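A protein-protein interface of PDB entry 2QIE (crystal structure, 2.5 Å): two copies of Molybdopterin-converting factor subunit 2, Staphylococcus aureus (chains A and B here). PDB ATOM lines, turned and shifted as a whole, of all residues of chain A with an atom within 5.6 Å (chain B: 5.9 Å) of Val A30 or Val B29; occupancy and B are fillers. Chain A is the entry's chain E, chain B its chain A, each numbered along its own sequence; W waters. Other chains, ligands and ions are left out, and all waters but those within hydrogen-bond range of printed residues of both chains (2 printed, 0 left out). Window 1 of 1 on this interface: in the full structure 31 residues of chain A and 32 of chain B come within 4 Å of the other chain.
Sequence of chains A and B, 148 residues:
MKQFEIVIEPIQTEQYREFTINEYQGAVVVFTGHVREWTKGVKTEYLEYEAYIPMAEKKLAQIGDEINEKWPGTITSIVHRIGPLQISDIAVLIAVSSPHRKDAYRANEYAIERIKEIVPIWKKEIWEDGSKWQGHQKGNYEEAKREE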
ATOM      1  N   ARG A  17       5.024   0.767  18.987  1.00  0.00           N
ATOM      2  CA  ARG A  17       4.047   1.539  18.227  1.00  0.00           C
ATOM      3  C   ARG A  17       2.653   1.012  18.542  1.00  0.00           C
ATOM      4  O   ARG A  17       1.762   1.779  18.897  1.00  0.00           O
ATOM      5  CB  ARG A  17       4.310   1.451  16.721  1.00  0.00           C
ATOM      6  CG  ARG A  17       3.263   2.182  15.865  1.00  0.00           C
ATOM      7  CD  ARG A  17       3.506   2.038  14.374  1.00  0.00           C
ATOM      8  NE  ARG A  17       4.706   2.760  13.973  1.00  0.00           N
ATOM      9  CZ  ARG A  17       5.928   2.238  13.891  1.00  0.00           C
ATOM     10  NH1 ARG A  17       6.150   0.959  14.178  1.00  0.00           N
ATOM     11  NH2 ARG A  17       6.947   3.006  13.523  1.00  0.00           N
ATOM     12  N   VAL A  28       1.770   8.846  15.552  1.00  0.00           N
ATOM     13  CA  VAL A  28       2.767   8.230  16.427  1.00  0.00           C
ATOM     14  C   VAL A  28       4.146   8.687  15.967  1.00  0.00           C
ATOM     15  O   VAL A  28       4.445   8.712  14.771  1.00  0.00           O
ATOM     16  CB  VAL A  28       2.699   6.683  16.441  1.00  0.00           C
ATOM     17  CG1 VAL A  28       3.646   6.116  17.514  1.00  0.00           C
ATOM     18  CG2 VAL A  28       1.252   6.197  16.673  1.00  0.00           C
ATOM     19  N   VAL A  29       4.959   9.078  16.944  1.00  0.00           N
ATOM     20  CA  VAL A  29       6.354   9.389  16.726  1.00  0.00           C
ATOM     21  C   VAL A  29       7.168   8.414  17.546  1.00  0.00           C
ATOM     22  O   VAL A  29       6.958   8.282  18.757  1.00  0.00           O
ATOM     23  CB  VAL A  29       6.676  10.827  17.139  1.00  0.00           C
ATOM     24  CG1 VAL A  29       8.179  11.117  16.996  1.00  0.00           C
ATOM     25  CG2 VAL A  29       5.895  11.780  16.284  1.00  0.00           C
ATOM     26  N   VAL A  30       8.088   7.725  16.880  1.00  0.00           N
ATOM     27  CA  VAL A  30       9.034   6.825  17.548  1.00  0.00           C
ATOM     28  C   VAL A  30      10.437   7.388  17.359  1.00  0.00           C
ATOM     29  O   VAL A  30      10.799   7.763  16.260  1.00  0.00           O
ATOM     30  CB  VAL A  30       8.965   5.379  16.978  1.00  0.00           C
ATOM     31  CG1 VAL A  30      10.031   4.489  17.615  1.00  0.00           C
ATOM     32  CG2 VAL A  30       7.575   4.775  17.207  1.00  0.00           C
ATOM     33  N   PHE A  31      11.203   7.464  18.446  1.00  0.00           N
ATOM     34  CA  PHE A  31      12.608   7.884  18.408  1.00  0.00           C
ATOM     35  C   PHE A  31      13.448   6.710  18.851  1.00  0.00           C
ATOM     36  O   PHE A  31      13.127   6.071  19.846  1.00  0.00           O
ATOM     37  CB  PHE A  31      12.866   9.084  19.342  1.00  0.00           C
ATOM     38  CG  PHE A  31      14.337   9.338  19.635  1.00  0.00           C
ATOM     39  CD1 PHE A  31      15.096  10.168  18.813  1.00  0.00           C
ATOM     40  CD2 PHE A  31      14.957   8.751  20.736  1.00  0.00           C
ATOM     41  CE1 PHE A  31      16.442  10.392  19.068  1.00  0.00           C
ATOM     42  CE2 PHE A  31      16.311   8.962  20.992  1.00  0.00           C
ATOM     43  CZ  PHE A  31      17.051   9.789  20.163  1.00  0.00           C
ATOM     44  N   THR A  32      14.522   6.431  18.118  1.00  0.00           N
ATOM     45  CA  THR A  32      15.484   5.404  18.514  1.00  0.00           C
ATOM     46  C   THR A  32      16.886   5.990  18.608  1.00  0.00           C
ATOM     47  O   THR A  32      17.359   6.634  17.673  1.00  0.00           O
ATOM     48  CB  THR A  32      15.491   4.208  17.551  1.00  0.00           C
ATOM     49  OG1 THR A  32      15.601   4.675  16.210  1.00  0.00           O
ATOM     50  CG2 THR A  32      14.214   3.408  17.707  1.00  0.00           C
ATOM     51  N   LEU A  93      14.449   3.616  23.114  1.00  0.00           N
ATOM     52  CA  LEU A  93      13.304   3.812  22.251  1.00  0.00           C
ATOM     53  C   LEU A  93      12.194   4.490  23.020  1.00  0.00           C
ATOM     54  O   LEU A  93      11.813   4.043  24.101  1.00  0.00           O
ATOM     55  CB  LEU A  93      12.807   2.474  21.723  1.00  0.00           C
ATOM     56  CG  LEU A  93      11.683   2.513  20.687  1.00  0.00           C
ATOM     57  CD1 LEU A  93      11.790   1.312  19.796  1.00  0.00           C
ATOM     58  CD2 LEU A  93      10.308   2.556  21.324  1.00  0.00           C
ATOM     59  N   ILE A  94      11.675   5.561  22.428  1.00  0.00           N
ATOM     60  CA  ILE A  94      10.548   6.319  22.944  1.00  0.00           C
ATOM     61  C   ILE A  94       9.457   6.329  21.883  1.00  0.00           C
ATOM     62  O   ILE A  94       9.730   6.629  20.715  1.00  0.00           O
ATOM     63  CB  ILE A  94      10.943   7.772  23.208  1.00  0.00           C
ATOM     64  CG1 ILE A  94      12.072   7.848  24.235  1.00  0.00           C
ATOM     65  CG2 ILE A  94       9.735   8.570  23.684  1.00  0.00           C
ATOM     66  CD1 ILE A  94      12.796   9.191  24.256  1.00  0.00           C
ATOM     67  N   ALA A  95       8.232   6.012  22.299  1.00  0.00           N
ATOM     68  CA  ALA A  95       7.066   6.053  21.420  1.00  0.00           C
ATOM     69  C   ALA A  95       5.934   6.859  22.065  1.00  0.00           C
ATOM     70  O   ALA A  95       5.522   6.584  23.203  1.00  0.00           O
ATOM     71  CB  ALA A  95       6.598   4.656  21.083  1.00  0.00           C
ATOM     72  N   VAL A  96       5.454   7.868  21.333  1.00  0.00           N
ATOM     73  CA  VAL A  96       4.363   8.728  21.791  1.00  0.00           C
ATOM     74  C   VAL A  96       3.307   8.802  20.698  1.00  0.00           C
ATOM     75  O   VAL A  96       3.597   9.229  19.595  1.00  0.00           O
ATOM     76  CB  VAL A  96       4.834  10.171  22.103  1.00  0.00           C
ATOM     77  CG1 VAL A  96       3.701  10.976  22.720  1.00  0.00           C
ATOM     78  CG2 VAL A  96       6.036  10.172  23.021  1.00  0.00           C
ATOM     79  N   TYR A 105       5.289  14.984  18.476  1.00  0.00           N
ATOM     80  CA  TYR A 105       6.654  15.459  18.311  1.00  0.00           C
ATOM     81  C   TYR A 105       7.155  16.131  19.593  1.00  0.00           C
ATOM     82  O   TYR A 105       8.295  15.940  19.979  1.00  0.00           O
ATOM     83  CB  TYR A 105       6.758  16.431  17.145  1.00  0.00           C
ATOM     84  CG  TYR A 105       6.807  15.804  15.757  1.00  0.00           C
ATOM     85  CD1 TYR A 105       5.710  15.890  14.894  1.00  0.00           C
ATOM     86  CD2 TYR A 105       7.965  15.200  15.281  1.00  0.00           C
ATOM     87  CE1 TYR A 105       5.749  15.357  13.627  1.00  0.00           C
ATOM     88  CE2 TYR A 105       8.017  14.666  14.002  1.00  0.00           C
ATOM     89  CZ  TYR A 105       6.901  14.748  13.178  1.00  0.00           C
ATOM     90  OH  TYR A 105       6.930  14.219  11.904  1.00  0.00           O
ATOM     91  N   ASN A 108       7.613  13.541  22.659  1.00  0.00           N
ATOM     92  CA  ASN A 108       8.720  12.650  22.359  1.00  0.00           C
ATOM     93  C   ASN A 108      10.065  13.334  22.575  1.00  0.00           C
ATOM     94  O   ASN A 108      10.962  12.759  23.193  1.00  0.00           O
ATOM     95  CB  ASN A 108       8.616  12.096  20.935  1.00  0.00           C
ATOM     96  CG  ASN A 108       9.437  10.833  20.747  1.00  0.00           C
ATOM     97  OD1 ASN A 108      10.663  10.870  20.845  1.00  0.00           O
ATOM     98  ND2 ASN A 108       8.766   9.703  20.499  1.00  0.00           N
ATOM     99  N   ARG B  17      13.161   2.498   8.859  1.00  0.00           N
ATOM    100  CA  ARG B  17      14.187   2.803   9.847  1.00  0.00           C
ATOM    101  C   ARG B  17      15.518   2.258   9.378  1.00  0.00           C
ATOM    102  O   ARG B  17      16.488   2.992   9.324  1.00  0.00           O
ATOM    103  CB  ARG B  17      13.857   2.218  11.230  1.00  0.00           C
ATOM    104  CG  ARG B  17      14.961   2.426  12.275  1.00  0.00           C
ATOM    105  CD  ARG B  17      14.740   1.608  13.551  1.00  0.00           C
ATOM    106  NE  ARG B  17      13.782   2.247  14.453  1.00  0.00           N
ATOM    107  CZ  ARG B  17      12.448   2.137  14.384  1.00  0.00           C
ATOM    108  NH1 ARG B  17      11.842   1.398  13.446  1.00  0.00           N
ATOM    109  NH2 ARG B  17      11.698   2.784  15.267  1.00  0.00           N
ATOM    110  N   ALA B  27      20.508   9.105  15.828  1.00  0.00           N
ATOM    111  CA  ALA B  27      19.081   9.194  16.070  1.00  0.00           C
ATOM    112  C   ALA B  27      18.313   8.900  14.805  1.00  0.00           C
ATOM    113  O   ALA B  27      18.702   9.322  13.720  1.00  0.00           O
ATOM    114  CB  ALA B  27      18.736  10.555  16.547  1.00  0.00           C
ATOM    115  N   VAL B  28      17.223   8.167  14.963  1.00  0.00           N
ATOM    116  CA  VAL B  28      16.237   8.011  13.918  1.00  0.00           C
ATOM    117  C   VAL B  28      14.907   8.444  14.523  1.00  0.00           C
ATOM    118  O   VAL B  28      14.559   8.051  15.633  1.00  0.00           O
ATOM    119  CB  VAL B  28      16.133   6.560  13.419  1.00  0.00           C
ATOM    120  CG1 VAL B  28      15.103   6.447  12.292  1.00  0.00           C
ATOM    121  CG2 VAL B  28      17.476   6.077  12.942  1.00  0.00           C
ATOM    122  N   VAL B  29      14.185   9.284  13.791  1.00  0.00           N
ATOM    123  CA  VAL B  29      12.828   9.639  14.169  1.00  0.00           C
ATOM    124  C   VAL B  29      11.927   9.098  13.066  1.00  0.00           C
ATOM    125  O   VAL B  29      12.192   9.301  11.871  1.00  0.00           O
ATOM    126  CB  VAL B  29      12.683  11.166  14.344  1.00  0.00           C
ATOM    127  CG1 VAL B  29      11.235  11.563  14.588  1.00  0.00           C
ATOM    128  CG2 VAL B  29      13.571  11.642  15.499  1.00  0.00           C
ATOM    129  N   VAL B  30      10.900   8.360  13.470  1.00  0.00           N
ATOM    130  CA  VAL B  30       9.905   7.832  12.547  1.00  0.00           C
ATOM    131  C   VAL B  30       8.545   8.364  12.934  1.00  0.00           C
ATOM    132  O   VAL B  30       8.100   8.200  14.071  1.00  0.00           O
ATOM    133  CB  VAL B  30       9.825   6.276  12.559  1.00  0.00           C
ATOM    134  CG1 VAL B  30       8.691   5.782  11.634  1.00  0.00           C
ATOM    135  CG2 VAL B  30      11.153   5.661  12.139  1.00  0.00           C
ATOM    136  N   PHE B  31       7.877   8.973  11.962  1.00  0.00           N
ATOM    137  CA  PHE B  31       6.508   9.425  12.125  1.00  0.00           C
ATOM    138  C   PHE B  31       5.608   8.503  11.339  1.00  0.00           C
ATOM    139  O   PHE B  31       5.873   8.224  10.171  1.00  0.00           O
ATOM    140  CB  PHE B  31       6.361  10.870  11.640  1.00  0.00           C
ATOM    141  CG  PHE B  31       4.939  11.357  11.578  1.00  0.00           C
ATOM    142  CD1 PHE B  31       4.324  11.880  12.697  1.00  0.00           C
ATOM    143  CD2 PHE B  31       4.230  11.309  10.387  1.00  0.00           C
ATOM    144  CE1 PHE B  31       3.029  12.337  12.645  1.00  0.00           C
ATOM    145  CE2 PHE B  31       2.933  11.763  10.323  1.00  0.00           C
ATOM    146  CZ  PHE B  31       2.332  12.280  11.460  1.00  0.00           C
ATOM    147  N   ILE B  94       7.358   8.384   7.776  1.00  0.00           N
ATOM    148  CA  ILE B  94       8.473   9.287   7.534  1.00  0.00           C
ATOM    149  C   ILE B  94       9.604   8.873   8.451  1.00  0.00           C
ATOM    150  O   ILE B  94       9.452   8.886   9.657  1.00  0.00           O
ATOM    151  CB  ILE B  94       8.090  10.760   7.824  1.00  0.00           C
ATOM    152  CG1 ILE B  94       6.906  11.184   6.953  1.00  0.00           C
ATOM    153  CG2 ILE B  94       9.281  11.687   7.582  1.00  0.00           C
ATOM    154  CD1 ILE B  94       6.403  12.595   7.214  1.00  0.00           C
ATOM    155  N   ALA B  95      10.732   8.494   7.872  1.00  0.00           N
ATOM    156  CA  ALA B  95      11.897   8.097   8.649  1.00  0.00           C
ATOM    157  C   ALA B  95      13.032   9.030   8.320  1.00  0.00           C
ATOM    158  O   ALA B  95      13.352   9.244   7.145  1.00  0.00           O
ATOM    159  CB  ALA B  95      12.288   6.676   8.346  1.00  0.00           C
ATOM    160  N   VAL B  96      13.607   9.611   9.364  1.00  0.00           N
ATOM    161  CA  VAL B  96      14.777  10.457   9.246  1.00  0.00           C
ATOM    162  C   VAL B  96      15.835  10.006  10.251  1.00  0.00           C
ATOM    163  O   VAL B  96      15.558   9.922  11.450  1.00  0.00           O
ATOM    164  CB  VAL B  96      14.435  11.923   9.547  1.00  0.00           C
ATOM    165  CG1 VAL B  96      15.661  12.811   9.343  1.00  0.00           C
ATOM    166  CG2 VAL B  96      13.297  12.391   8.684  1.00  0.00           C
ATOM    167  N   SER B  97      17.028   9.716   9.748  1.00  0.00           N
ATOM    168  CA  SER B  97      18.218   9.517  10.575  1.00  0.00           C
ATOM    169  C   SER B  97      19.120  10.739  10.495  1.00  0.00           C
ATOM    170  O   SER B  97      19.153  11.418   9.479  1.00  0.00           O
ATOM    171  CB  SER B  97      19.022   8.296  10.115  1.00  0.00           C
ATOM    172  OG  SER B  97      19.615   8.526   8.842  1.00  0.00           O
ATOM    173  N   ARG B 101      20.204  14.230  17.466  1.00  0.00           N
ATOM    174  CA  ARG B 101      18.768  14.046  17.661  1.00  0.00           C
ATOM    175  C   ARG B 101      17.905  15.237  17.236  1.00  0.00           C
ATOM    176  O   ARG B 101      16.839  15.038  16.669  1.00  0.00           O
ATOM    177  CB  ARG B 101      18.456  13.664  19.116  1.00  0.00           C
ATOM    178  CG  ARG B 101      18.681  14.754  20.124  1.00  0.00           C
ATOM    179  CD  ARG B 101      18.013  14.454  21.441  1.00  0.00           C
ATOM    180  NE  ARG B 101      18.399  15.445  22.440  1.00  0.00           N
ATOM    181  CZ  ARG B 101      19.579  15.474  23.055  1.00  0.00           C
ATOM    182  NH1 ARG B 101      20.498  14.556  22.786  1.00  0.00           N
ATOM    183  NH2 ARG B 101      19.847  16.421  23.947  1.00  0.00           N
ATOM    184  N   ALA B 104      17.200  15.300  13.535  1.00  0.00           N
ATOM    185  CA  ALA B 104      16.257  14.212  13.265  1.00  0.00           C
ATOM    186  C   ALA B 104      14.813  14.612  13.522  1.00  0.00           C
ATOM    187  O   ALA B 104      13.964  14.396  12.658  1.00  0.00           O
ATOM    188  CB  ALA B 104      16.603  12.982  14.076  1.00  0.00           C
ATOM    189  N   TYR B 105      14.530  15.182  14.695  1.00  0.00           N
ATOM    190  CA  TYR B 105      13.178  15.705  14.993  1.00  0.00           C
ATOM    191  C   TYR B 105      12.743  16.893  14.089  1.00  0.00           C
ATOM    192  O   TYR B 105      11.596  16.944  13.629  1.00  0.00           O
ATOM    193  CB  TYR B 105      13.076  16.180  16.436  1.00  0.00           C
ATOM    194  CG  TYR B 105      12.995  15.123  17.516  1.00  0.00           C
ATOM    195  CD1 TYR B 105      14.070  14.896  18.363  1.00  0.00           C
ATOM    196  CD2 TYR B 105      11.830  14.399  17.735  1.00  0.00           C
ATOM    197  CE1 TYR B 105      14.002  13.964  19.382  1.00  0.00           C
ATOM    198  CE2 TYR B 105      11.752  13.451  18.760  1.00  0.00           C
ATOM    199  CZ  TYR B 105      12.844  13.241  19.584  1.00  0.00           C
ATOM    200  OH  TYR B 105      12.805  12.318  20.616  1.00  0.00           O
ATOM    201  N   ASN B 108      12.182  15.642  10.396  1.00  0.00           N
ATOM    202  CA  ASN B 108      10.977  14.823  10.265  1.00  0.00           C
ATOM    203  C   ASN B 108       9.741  15.727  10.252  1.00  0.00           C
ATOM    204  O   ASN B 108       8.892  15.624   9.370  1.00  0.00           O
ATOM    205  CB  ASN B 108      10.914  13.777  11.383  1.00  0.00           C
ATOM    206  CG  ASN B 108       9.960  12.627  11.069  1.00  0.00           C
ATOM    207  OD1 ASN B 108       8.757  12.784  11.166  1.00  0.00           O
ATOM    208  ND2 ASN B 108      10.500  11.469  10.729  1.00  0.00           N
HETATM  209  O   HOH W   1      13.130   5.607  15.521  1.00  0.00           O
HETATM  210  O   HOH W   2       6.079   6.079  14.179  1.00  0.00           O
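Val A28 touches Phe B31, and with the chains exchanged Phe A31 touches Val B28.
Val A29 touches Val B30, and with the chains exchanged Val A30 touches Val B29.
Phe A31 touches Tyr B105, and with the chains exchanged Tyr A105 touches Phe B31.
Tyr A105 touches Asn B108, and with the chains exchanged Asn A108 touches Tyr B105.
Val A30 touches just these residues of chain B: Arg B17, Val B28, Val B29 and Val B30.
Val B29 touches just these residues of chain A: Val A29, Val A30 and Phe A31.
Of the printed residues of chain B, Tyr A105 touches Phe B31 and Asn B108.
Printed residues of chain B within 4 Å of Val A29: Val B29, Val B30 and Phe B31.
Printed residues of chain B within 4 Å of Asn A108: Tyr B105 (2.6 Å).
Printed residues of chain B within 4 Å of Val A28: Val B30 (3.8 Å) and Phe B31 (3.4 Å).
Of the printed residues of chain B, Arg A17 touches Val B30 (3.8 Å).
Ala B104 touches none of the printed residues of chain A.
Val B96 touches none of the printed residues of chain A.
The nearest residue of chain B that does not touch Val A30 is Phe B31 (5.1 Å).
The nearest printed residue of chain B that does not touch Val A28 is Asn B108 (6.9 Å).
Printed residues of chain B that touch a printed residue of chain A: Arg B17, Ala B27, Val B28, Val B29, Val B30, Phe B31, Arg B101, Tyr B105 and Asn B108.
Hydrophobic or aromatic side chains of chain B within 4 Å of the printed part of chain A: Ala B27, Val B28, Val B29, Val B30, Phe B31 and Tyr B105.
Among the printed residues, 21 pairs touch across the chains.
The backbone NH (N) of Val A29 lies within hydrogen-bond range of the backbone carbonyl oxygen (O) of Val A96 (3.0 Å).
The backbone NH (N) of Phe B31 sits at hydrogen-bond distance from the backbone carbonyl oxygen (O) of Ile B94, 2.8 Å away.
The backbone carbonyl oxygen (O) of Ile A94 lies within hydrogen-bond range of the side-chain amide nitrogen (ND2) of Asn A108.
The backbone carbonyl oxygen (O) of Val B96 sits at hydrogen-bond distance from the backbone NH (N) of Val B29, at 2.8 Å.
ND2 of Asn A108 sits at hydrogen-bond distance from O of Val A29, 2.9 Å away.
ND2 of Asn B108 is in hydrogen-bond range of O of Val B29 (3.0 Å).
O of Val B30 is in hydrogen-bond range of N of Val A30 (2.8 Å).
The side-chain amide oxygen (OD1) of Asn B108 sits at hydrogen-bond distance from the side-chain hydroxyl (OH) of Tyr A105 (2.4 Å).
The side-chain amide oxygen of Asn A108 lies within hydrogen-bond range of the side-chain hydroxyl of Tyr B105, at 2.6 Å.
The backbone NH of Thr A32 lies within hydrogen-bond range of the backbone carbonyl oxygen of Val B28 (3.0 Å).
Water W1 lies within hydrogen-bond range of the side-chain hydroxyl of Thr A32 (2.7 Å), the backbone carbonyl oxygen of Val B28 (2.8 Å), the guanidinium group of Arg B17 (3.2 Å) and the backbone carbonyl oxygen of Val A30 (3.3 Å).
Water W2 lies within hydrogen-bond range of the backbone carbonyl oxygen of Val B30 (2.9 Å), the backbone carbonyl oxygen of Val A28 (3.2 Å) and the guanidinium group of Arg A17 (3.3 Å).
Among the printed residues, merely in contact across the chains: Val A30 with Arg B17, Val A29 with Val B30, Phe A31 with Val B28, Tyr A105 with Phe B31, Phe A31 with Ala B27, Val A28 with Phe B31, Val A30 with Val B29, Phe A31 with Tyr B105, Thr A32 with Ala B27, Thr A32 with Arg B17, Val A28 with Val B30, Arg A17 with Val B30, Val A30 with Val B28, Phe A31 with Arg B101, Val A29 with Val B29, Val A29 with Phe B31 and Phe A31 with Val B29.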
